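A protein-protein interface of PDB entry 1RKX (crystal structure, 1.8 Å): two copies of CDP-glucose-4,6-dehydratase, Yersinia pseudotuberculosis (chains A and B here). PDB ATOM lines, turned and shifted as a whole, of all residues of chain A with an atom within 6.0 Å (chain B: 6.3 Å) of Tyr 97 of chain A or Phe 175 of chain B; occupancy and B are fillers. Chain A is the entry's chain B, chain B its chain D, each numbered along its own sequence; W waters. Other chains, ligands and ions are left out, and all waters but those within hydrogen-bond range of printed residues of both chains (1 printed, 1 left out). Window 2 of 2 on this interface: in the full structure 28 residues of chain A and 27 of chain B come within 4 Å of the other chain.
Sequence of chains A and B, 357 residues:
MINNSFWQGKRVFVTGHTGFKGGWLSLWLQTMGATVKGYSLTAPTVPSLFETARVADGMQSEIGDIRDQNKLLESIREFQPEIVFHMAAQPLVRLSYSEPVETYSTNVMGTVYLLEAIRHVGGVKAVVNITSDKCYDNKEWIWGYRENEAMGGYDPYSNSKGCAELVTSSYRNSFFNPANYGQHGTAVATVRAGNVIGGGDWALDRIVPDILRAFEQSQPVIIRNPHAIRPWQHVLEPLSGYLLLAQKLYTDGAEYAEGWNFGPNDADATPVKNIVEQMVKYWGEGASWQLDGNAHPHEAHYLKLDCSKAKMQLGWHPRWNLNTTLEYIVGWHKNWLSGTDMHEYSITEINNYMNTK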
ATOM      1  N   LEU A  92      27.183 -12.519  20.564  1.00  0.00           N
ATOM      2  CA  LEU A  92      26.047 -12.900  19.739  1.00  0.00           C
ATOM      3  C   LEU A  92      25.368 -14.217  20.054  1.00  0.00           C
ATOM      4  O   LEU A  92      26.006 -15.273  20.114  1.00  0.00           O
ATOM      5  CB  LEU A  92      26.461 -12.911  18.268  1.00  0.00           C
ATOM      6  CG  LEU A  92      27.131 -11.633  17.766  1.00  0.00           C
ATOM      7  CD1 LEU A  92      27.517 -11.813  16.307  1.00  0.00           C
ATOM      8  CD2 LEU A  92      26.190 -10.445  17.938  1.00  0.00           C
ATOM      9  N   VAL A  93      24.057 -14.136  20.232  1.00  0.00           N
ATOM     10  CA  VAL A  93      23.252 -15.317  20.500  1.00  0.00           C
ATOM     11  C   VAL A  93      23.329 -16.212  19.266  1.00  0.00           C
ATOM     12  O   VAL A  93      23.707 -17.377  19.357  1.00  0.00           O
ATOM     13  CB  VAL A  93      21.776 -14.938  20.746  1.00  0.00           C
ATOM     14  CG1 VAL A  93      20.913 -16.195  20.833  1.00  0.00           C
ATOM     15  CG2 VAL A  93      21.661 -14.132  22.022  1.00  0.00           C
ATOM     16  N   ARG A  94      22.975 -15.656  18.111  1.00  0.00           N
ATOM     17  CA  ARG A  94      22.994 -16.413  16.866  1.00  0.00           C
ATOM     18  C   ARG A  94      24.291 -17.195  16.683  1.00  0.00           C
ATOM     19  O   ARG A  94      24.271 -18.409  16.484  1.00  0.00           O
ATOM     20  CB  ARG A  94      22.790 -15.478  15.671  1.00  0.00           C
ATOM     21  CG  ARG A  94      22.831 -16.182  14.323  1.00  0.00           C
ATOM     22  CD  ARG A  94      22.646 -15.201  13.175  1.00  0.00           C
ATOM     23  NE  ARG A  94      22.791 -15.848  11.873  1.00  0.00           N
ATOM     24  CZ  ARG A  94      22.718 -15.213  10.707  1.00  0.00           C
ATOM     25  NH1 ARG A  94      22.500 -13.904  10.674  1.00  0.00           N
ATOM     26  NH2 ARG A  94      22.870 -15.883   9.574  1.00  0.00           N
ATOM     27  N   LEU A  95      25.419 -16.495  16.753  1.00  0.00           N
ATOM     28  CA  LEU A  95      26.720 -17.134  16.591  1.00  0.00           C
ATOM     29  C   LEU A  95      27.004 -18.202  17.656  1.00  0.00           C
ATOM     30  O   LEU A  95      27.719 -19.172  17.388  1.00  0.00           O
ATOM     31  CB  LEU A  95      27.832 -16.080  16.626  1.00  0.00           C
ATOM     32  CG  LEU A  95      29.251 -16.569  16.320  1.00  0.00           C
ATOM     33  CD1 LEU A  95      29.273 -17.253  14.955  1.00  0.00           C
ATOM     34  CD2 LEU A  95      30.214 -15.386  16.334  1.00  0.00           C
ATOM     35  N   SER A  96      26.459 -18.023  18.858  1.00  0.00           N
ATOM     36  CA  SER A  96      26.703 -18.986  19.929  1.00  0.00           C
ATOM     37  C   SER A  96      26.120 -20.358  19.599  1.00  0.00           C
ATOM     38  O   SER A  96      26.624 -21.374  20.071  1.00  0.00           O
ATOM     39  CB  SER A  96      26.152 -18.474  21.279  1.00  0.00           C
ATOM     40  OG  SER A  96      24.749 -18.633  21.413  1.00  0.00           O
ATOM     41  N   TYR A  97      25.070 -20.400  18.781  1.00  0.00           N
ATOM     42  CA  TYR A  97      24.489 -21.685  18.411  1.00  0.00           C
ATOM     43  C   TYR A  97      25.409 -22.377  17.414  1.00  0.00           C
ATOM     44  O   TYR A  97      25.460 -23.602  17.346  1.00  0.00           O
ATOM     45  CB  TYR A  97      23.102 -21.514  17.775  1.00  0.00           C
ATOM     46  CG  TYR A  97      21.982 -21.286  18.765  1.00  0.00           C
ATOM     47  CD1 TYR A  97      21.429 -20.020  18.942  1.00  0.00           C
ATOM     48  CD2 TYR A  97      21.471 -22.338  19.518  1.00  0.00           C
ATOM     49  CE1 TYR A  97      20.386 -19.810  19.846  1.00  0.00           C
ATOM     50  CE2 TYR A  97      20.431 -22.139  20.427  1.00  0.00           C
ATOM     51  CZ  TYR A  97      19.893 -20.875  20.583  1.00  0.00           C
ATOM     52  OH  TYR A  97      18.847 -20.683  21.459  1.00  0.00           O
ATOM     53  N   SER A  98      26.131 -21.575  16.640  1.00  0.00           N
ATOM     54  CA  SER A  98      27.048 -22.097  15.634  1.00  0.00           C
ATOM     55  C   SER A  98      28.422 -22.397  16.226  1.00  0.00           C
ATOM     56  O   SER A  98      29.103 -23.329  15.801  1.00  0.00           O
ATOM     57  CB  SER A  98      27.193 -21.089  14.491  1.00  0.00           C
ATOM     58  OG  SER A  98      28.190 -21.503  13.578  1.00  0.00           O
ATOM     59  N   GLU A  99      28.823 -21.603  17.211  1.00  0.00           N
ATOM     60  CA  GLU A  99      30.122 -21.780  17.845  1.00  0.00           C
ATOM     61  C   GLU A  99      29.988 -21.769  19.363  1.00  0.00           C
ATOM     62  O   GLU A  99      30.489 -20.868  20.040  1.00  0.00           O
ATOM     63  CB  GLU A  99      31.071 -20.672  17.379  1.00  0.00           C
ATOM     64  CG  GLU A  99      31.248 -20.650  15.862  1.00  0.00           C
ATOM     65  CD  GLU A  99      32.082 -19.482  15.367  1.00  0.00           C
ATOM     66  OE1 GLU A  99      32.252 -19.356  14.136  1.00  0.00           O
ATOM     67  OE2 GLU A  99      32.569 -18.690  16.200  1.00  0.00           O
ATOM     68  N   PRO A 100      29.309 -22.784  19.922  1.00  0.00           N
ATOM     69  CA  PRO A 100      29.135 -22.840  21.372  1.00  0.00           C
ATOM     70  C   PRO A 100      30.443 -22.911  22.157  1.00  0.00           C
ATOM     71  O   PRO A 100      30.612 -22.208  23.151  1.00  0.00           O
ATOM     72  CB  PRO A 100      28.253 -24.078  21.568  1.00  0.00           C
ATOM     73  CG  PRO A 100      28.575 -24.939  20.376  1.00  0.00           C
ATOM     74  CD  PRO A 100      28.633 -23.918  19.264  1.00  0.00           C
ATOM     75  N   THR A 103      32.253 -19.718  22.357  1.00  0.00           N
ATOM     76  CA  THR A 103      31.497 -18.810  23.210  1.00  0.00           C
ATOM     77  C   THR A 103      31.831 -19.062  24.684  1.00  0.00           C
ATOM     78  O   THR A 103      32.082 -18.114  25.423  1.00  0.00           O
ATOM     79  CB  THR A 103      29.984 -18.964  22.979  1.00  0.00           C
ATOM     80  OG1 THR A 103      29.667 -18.540  21.646  1.00  0.00           O
ATOM     81  CG2 THR A 103      29.189 -18.118  23.979  1.00  0.00           C
ATOM     82  N   TYR A 154      19.347 -19.849  28.381  1.00  0.00           N
ATOM     83  CA  TYR A 154      18.901 -20.862  27.430  1.00  0.00           C
ATOM     84  C   TYR A 154      19.979 -21.234  26.418  1.00  0.00           C
ATOM     85  O   TYR A 154      20.447 -22.364  26.359  1.00  0.00           O
ATOM     86  CB  TYR A 154      17.669 -20.341  26.685  1.00  0.00           C
ATOM     87  CG  TYR A 154      16.983 -21.370  25.818  1.00  0.00           C
ATOM     88  CD1 TYR A 154      16.172 -22.354  26.384  1.00  0.00           C
ATOM     89  CD2 TYR A 154      17.134 -21.355  24.433  1.00  0.00           C
ATOM     90  CE1 TYR A 154      15.524 -23.297  25.588  1.00  0.00           C
ATOM     91  CE2 TYR A 154      16.491 -22.296  23.630  1.00  0.00           C
ATOM     92  CZ  TYR A 154      15.689 -23.261  24.215  1.00  0.00           C
ATOM     93  OH  TYR A 154      15.043 -24.190  23.430  1.00  0.00           O
ATOM     94  N   ASP A 155      20.351 -20.261  25.602  1.00  0.00           N
ATOM     95  CA  ASP A 155      21.362 -20.450  24.570  1.00  0.00           C
ATOM     96  C   ASP A 155      22.764 -20.359  25.175  1.00  0.00           C
ATOM     97  O   ASP A 155      22.938 -19.828  26.273  1.00  0.00           O
ATOM     98  CB  ASP A 155      21.213 -19.352  23.530  1.00  0.00           C
ATOM     99  CG  ASP A 155      21.356 -17.970  24.142  1.00  0.00           C
ATOM    100  OD1 ASP A 155      20.384 -17.486  24.763  1.00  0.00           O
ATOM    101  OD2 ASP A 155      22.452 -17.382  24.022  1.00  0.00           O
ATOM    102  N   PRO A 156      23.784 -20.863  24.457  1.00  0.00           N
ATOM    103  CA  PRO A 156      25.172 -20.836  24.935  1.00  0.00           C
ATOM    104  C   PRO A 156      25.677 -19.448  25.336  1.00  0.00           C
ATOM    105  O   PRO A 156      26.425 -19.315  26.306  1.00  0.00           O
ATOM    106  CB  PRO A 156      25.947 -21.427  23.763  1.00  0.00           C
ATOM    107  CG  PRO A 156      24.963 -22.429  23.201  1.00  0.00           C
ATOM    108  CD  PRO A 156      23.682 -21.628  23.199  1.00  0.00           C
ATOM    109  N   GLU B 116      30.081 -31.267  23.265  1.00  0.00           N
ATOM    110  CA  GLU B 116      30.298 -30.895  21.866  1.00  0.00           C
ATOM    111  C   GLU B 116      30.632 -32.145  21.041  1.00  0.00           C
ATOM    112  O   GLU B 116      30.147 -32.307  19.921  1.00  0.00           O
ATOM    113  CB  GLU B 116      31.436 -29.881  21.756  1.00  0.00           C
ATOM    114  CG  GLU B 116      31.680 -29.332  20.354  1.00  0.00           C
ATOM    115  CD  GLU B 116      30.542 -28.460  19.841  1.00  0.00           C
ATOM    116  OE1 GLU B 116      29.603 -28.158  20.611  1.00  0.00           O
ATOM    117  OE2 GLU B 116      30.598 -28.068  18.658  1.00  0.00           O
ATOM    118  N   ARG B 119      27.547 -34.131  20.520  1.00  0.00           N
ATOM    119  CA  ARG B 119      26.708 -33.422  19.563  1.00  0.00           C
ATOM    120  C   ARG B 119      27.086 -33.775  18.126  1.00  0.00           C
ATOM    121  O   ARG B 119      26.220 -34.059  17.292  1.00  0.00           O
ATOM    122  CB  ARG B 119      26.859 -31.914  19.788  1.00  0.00           C
ATOM    123  CG  ARG B 119      26.009 -31.030  18.905  1.00  0.00           C
ATOM    124  CD  ARG B 119      25.959 -29.612  19.466  1.00  0.00           C
ATOM    125  NE  ARG B 119      27.083 -28.766  19.072  1.00  0.00           N
ATOM    126  CZ  ARG B 119      27.118 -28.054  17.949  1.00  0.00           C
ATOM    127  NH1 ARG B 119      26.091 -28.093  17.109  1.00  0.00           N
ATOM    128  NH2 ARG B 119      28.167 -27.288  17.676  1.00  0.00           N
ATOM    129  N   SER B 170      22.137 -25.545  28.979  1.00  0.00           N
ATOM    130  CA  SER B 170      22.129 -24.841  27.701  1.00  0.00           C
ATOM    131  C   SER B 170      22.352 -25.784  26.521  1.00  0.00           C
ATOM    132  O   SER B 170      21.680 -25.659  25.498  1.00  0.00           O
ATOM    133  CB  SER B 170      23.194 -23.744  27.666  1.00  0.00           C
ATOM    134  OG  SER B 170      23.210 -23.115  26.390  1.00  0.00           O
ATOM    135  N   TYR B 171      23.303 -26.706  26.647  1.00  0.00           N
ATOM    136  CA  TYR B 171      23.552 -27.650  25.555  1.00  0.00           C
ATOM    137  C   TYR B 171      22.295 -28.465  25.275  1.00  0.00           C
ATOM    138  O   TYR B 171      21.939 -28.692  24.114  1.00  0.00           O
ATOM    139  CB  TYR B 171      24.724 -28.586  25.878  1.00  0.00           C
ATOM    140  CG  TYR B 171      25.997 -28.208  25.153  1.00  0.00           C
ATOM    141  CD1 TYR B 171      26.783 -27.134  25.585  1.00  0.00           C
ATOM    142  CD2 TYR B 171      26.393 -28.892  24.000  1.00  0.00           C
ATOM    143  CE1 TYR B 171      27.926 -26.750  24.883  1.00  0.00           C
ATOM    144  CE2 TYR B 171      27.532 -28.517  23.293  1.00  0.00           C
ATOM    145  CZ  TYR B 171      28.294 -27.447  23.735  1.00  0.00           C
ATOM    146  OH  TYR B 171      29.407 -27.062  23.021  1.00  0.00           O
ATOM    147  N   ARG B 172      21.611 -28.887  26.337  1.00  0.00           N
ATOM    148  CA  ARG B 172      20.388 -29.670  26.180  1.00  0.00           C
ATOM    149  C   ARG B 172      19.316 -28.848  25.469  1.00  0.00           C
ATOM    150  O   ARG B 172      18.714 -29.295  24.492  1.00  0.00           O
ATOM    151  CB  ARG B 172      19.863 -30.128  27.546  1.00  0.00           C
ATOM    152  CG  ARG B 172      18.545 -30.912  27.481  1.00  0.00           C
ATOM    153  CD  ARG B 172      18.203 -31.531  28.830  1.00  0.00           C
ATOM    154  NE  ARG B 172      18.153 -30.514  29.872  1.00  0.00           N
ATOM    155  CZ  ARG B 172      18.659 -30.650  31.093  1.00  0.00           C
ATOM    156  NH1 ARG B 172      19.266 -31.773  31.452  1.00  0.00           N
ATOM    157  NH2 ARG B 172      18.557 -29.648  31.958  1.00  0.00           N
ATOM    158  N   ASN B 173      19.087 -27.639  25.960  1.00  0.00           N
ATOM    159  CA  ASN B 173      18.080 -26.758  25.374  1.00  0.00           C
ATOM    160  C   ASN B 173      18.382 -26.379  23.931  1.00  0.00           C
ATOM    161  O   ASN B 173      17.478 -26.311  23.092  1.00  0.00           O
ATOM    162  CB  ASN B 173      17.960 -25.480  26.209  1.00  0.00           C
ATOM    163  CG  ASN B 173      17.186 -25.691  27.495  1.00  0.00           C
ATOM    164  OD1 ASN B 173      17.235 -24.861  28.405  1.00  0.00           O
ATOM    165  ND2 ASN B 173      16.454 -26.796  27.574  1.00  0.00           N
ATOM    166  N   SER B 174      19.655 -26.134  23.645  1.00  0.00           N
ATOM    167  CA  SER B 174      20.071 -25.715  22.316  1.00  0.00           C
ATOM    168  C   SER B 174      20.297 -26.827  21.301  1.00  0.00           C
ATOM    169  O   SER B 174      19.925 -26.682  20.132  1.00  0.00           O
ATOM    170  CB  SER B 174      21.355 -24.885  22.409  1.00  0.00           C
ATOM    171  OG  SER B 174      21.212 -23.813  23.331  1.00  0.00           O
ATOM    172  N   PHE B 175      20.889 -27.934  21.739  1.00  0.00           N
ATOM    173  CA  PHE B 175      21.215 -29.014  20.814  1.00  0.00           C
ATOM    174  C   PHE B 175      20.585 -30.382  21.051  1.00  0.00           C
ATOM    175  O   PHE B 175      20.588 -31.219  20.151  1.00  0.00           O
ATOM    176  CB  PHE B 175      22.736 -29.156  20.758  1.00  0.00           C
ATOM    177  CG  PHE B 175      23.461 -27.842  20.603  1.00  0.00           C
ATOM    178  CD1 PHE B 175      24.272 -27.358  21.625  1.00  0.00           C
ATOM    179  CD2 PHE B 175      23.316 -27.080  19.442  1.00  0.00           C
ATOM    180  CE1 PHE B 175      24.931 -26.135  21.497  1.00  0.00           C
ATOM    181  CE2 PHE B 175      23.972 -25.856  19.302  1.00  0.00           C
ATOM    182  CZ  PHE B 175      24.785 -25.383  20.340  1.00  0.00           C
ATOM    183  N   PHE B 176      20.060 -30.620  22.248  1.00  0.00           N
ATOM    184  CA  PHE B 176      19.435 -31.904  22.559  1.00  0.00           C
ATOM    185  C   PHE B 176      18.048 -31.640  23.148  1.00  0.00           C
ATOM    186  O   PHE B 176      17.636 -32.278  24.117  1.00  0.00           O
ATOM    187  CB  PHE B 176      20.283 -32.688  23.571  1.00  0.00           C
ATOM    188  CG  PHE B 176      21.728 -32.851  23.171  1.00  0.00           C
ATOM    189  CD1 PHE B 176      22.744 -32.280  23.941  1.00  0.00           C
ATOM    190  CD2 PHE B 176      22.079 -33.585  22.038  1.00  0.00           C
ATOM    191  CE1 PHE B 176      24.087 -32.440  23.589  1.00  0.00           C
ATOM    192  CE2 PHE B 176      23.418 -33.753  21.677  1.00  0.00           C
ATOM    193  CZ  PHE B 176      24.426 -33.179  22.454  1.00  0.00           C
ATOM    194  N   ASN B 177      17.333 -30.701  22.539  1.00  0.00           N
ATOM    195  CA  ASN B 177      16.006 -30.302  22.994  1.00  0.00           C
ATOM    196  C   ASN B 177      14.951 -31.402  22.858  1.00  0.00           C
ATOM    197  O   ASN B 177      14.885 -32.089  21.842  1.00  0.00           O
ATOM    198  CB  ASN B 177      15.557 -29.057  22.227  1.00  0.00           C
ATOM    199  CG  ASN B 177      14.373 -28.369  22.875  1.00  0.00           C
ATOM    200  OD1 ASN B 177      13.256 -28.892  22.877  1.00  0.00           O
ATOM    201  ND2 ASN B 177      14.614 -27.187  23.439  1.00  0.00           N
ATOM    202  N   ASN B 180      12.974 -31.878  19.805  1.00  0.00           N
ATOM    203  CA  ASN B 180      13.712 -32.401  18.659  1.00  0.00           C
ATOM    204  C   ASN B 180      14.306 -33.776  18.937  1.00  0.00           C
ATOM    205  O   ASN B 180      15.125 -34.264  18.163  1.00  0.00           O
ATOM    206  CB  ASN B 180      14.853 -31.452  18.269  1.00  0.00           C
ATOM    207  CG  ASN B 180      14.363 -30.070  17.893  1.00  0.00           C
ATOM    208  OD1 ASN B 180      13.474 -29.923  17.055  1.00  0.00           O
ATOM    209  ND2 ASN B 180      14.947 -29.044  18.507  1.00  0.00           N
ATOM    210  N   HIS B 184      17.531 -35.961  17.148  1.00  0.00           N
ATOM    211  CA  HIS B 184      18.849 -36.266  17.710  1.00  0.00           C
ATOM    212  C   HIS B 184      18.890 -37.516  18.588  1.00  0.00           C
ATOM    213  O   HIS B 184      19.931 -38.178  18.677  1.00  0.00           O
ATOM    214  CB  HIS B 184      19.384 -35.046  18.479  1.00  0.00           C
ATOM    215  CG  HIS B 184      18.515 -34.613  19.620  1.00  0.00           C
ATOM    216  ND1 HIS B 184      18.459 -35.294  20.816  1.00  0.00           N
ATOM    217  CD2 HIS B 184      17.660 -33.570  19.741  1.00  0.00           C
ATOM    218  CE1 HIS B 184      17.609 -34.689  21.627  1.00  0.00           C
ATOM    219  NE2 HIS B 184      17.110 -33.640  20.998  1.00  0.00           N
HETATM  220  O   HOH W   1      15.919 -24.753  20.775  1.00  0.00           O
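The side-chain hydroxyl (OG) of Ser 170 of chain B lies close to the backbone carbonyl oxygen (O) of Asp 155 of chain A (3.3 Å). The side-chain hydroxyl (OG) of Ser 170 of chain B lies close to the backbone nitrogen (N) of Pro 156 of chain A (3.0 Å). The side-chain amide nitrogen (ND2) of Asn 177 of chain B sits at hydrogen-bond distance from the side-chain hydroxyl (OH) of Tyr 154 of chain A. O of Tyr 154 of chain A is in hydrogen-bond range of OG of Ser 170 of chain B, 2.9 Å away. The backbone carbonyl oxygen (O) of Tyr 154 of chain A lies within hydrogen-bond range of the side-chain hydroxyl (OG) of Ser 174 of chain B (3.4 Å). OH of Tyr 154 of chain A lies within hydrogen-bond range of O of Asn 173 of chain B (3.2 Å).
NE2 of His 184 of chain B lies within hydrogen-bond range of O of Asn 177 of chain B, at 2.8 Å. NH2 of Arg 119 of chain B lies within salt-bridge range of OE2 of Glu 116 of chain B (2.7 Å). The backbone carbonyl oxygen (O) of Arg 172 of chain B sits at hydrogen-bond distance from the backbone NH (N) of Asn 177 of chain B, at 2.8 Å. O of Tyr 171 of chain B lies within hydrogen-bond range of N of Phe 176 of chain B. OG of Ser 174 of chain B lies within hydrogen-bond range of O of Ser 170 of chain B (2.9 Å). The backbone carbonyl oxygen of Asn 173 of chain B lies within hydrogen-bond range of the side-chain amide nitrogen of Asn 177 of chain B (3.0 Å).
Among the printed residues, merely in contact across the chains: Pro 156 of chain A with Ser 174 of chain B (3.3 Å), Tyr 97 of chain A with Phe 175 of chain B (3.3 Å), Pro 100 of chain A with Glu 116 of chain B (3.4 Å), Tyr 97 of chain A with Ser 174 of chain B (3.4 Å), Pro 100 of chain A with Tyr 171 of chain B (3.5 Å), Asp 155 of chain A with Ser 174 of chain B (3.6 Å), Pro 100 of chain A with Arg 119 of chain B (3.6 Å) and Pro 100 of chain A with Phe 175 of chain B (3.8 Å).
Ser 96 of chain A touches none of the printed residues of chain B. Of chain B, only Ser 174 and Phe 175 come within 4 Å of Tyr 97 of chain A. Of the printed residues of chain B, Tyr 154 of chain A touches Ser 170 (2.9 Å), Asn 173 (3.2 Å), Ser 174 (3.4 Å) and Asn 177 (3.0 Å). Of the printed residues of chain A, Tyr 171 of chain B touches Pro 100. Of chain A, only Tyr 97 (3.3 Å) and Pro 100 (3.8 Å) come within 4 Å of Phe 175 of chain B. Printed residues of chain A within 4 Å of Asn 177 of chain B: Tyr 154. The nearest residue of chain B that does not touch Tyr 97 of chain A is Arg 119 of chain B (4.5 Å). The nearest printed residue of chain A that does not touch Asn 173 of chain B is Tyr 97 of chain A (5.8 Å).
Hydrophobic or aromatic side chains of chain B within 4 Å of the printed part of chain A: Tyr 171 and Phe 175. Among the printed residues, no Asp or Glu carboxylate lies within 4 Å of a Lys or Arg side-chain nitrogen of the other chain.
No position is printed for both chains.
Water W1 bridges OH of Tyr 154 of chain A and O of Asn 173 of chain B.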
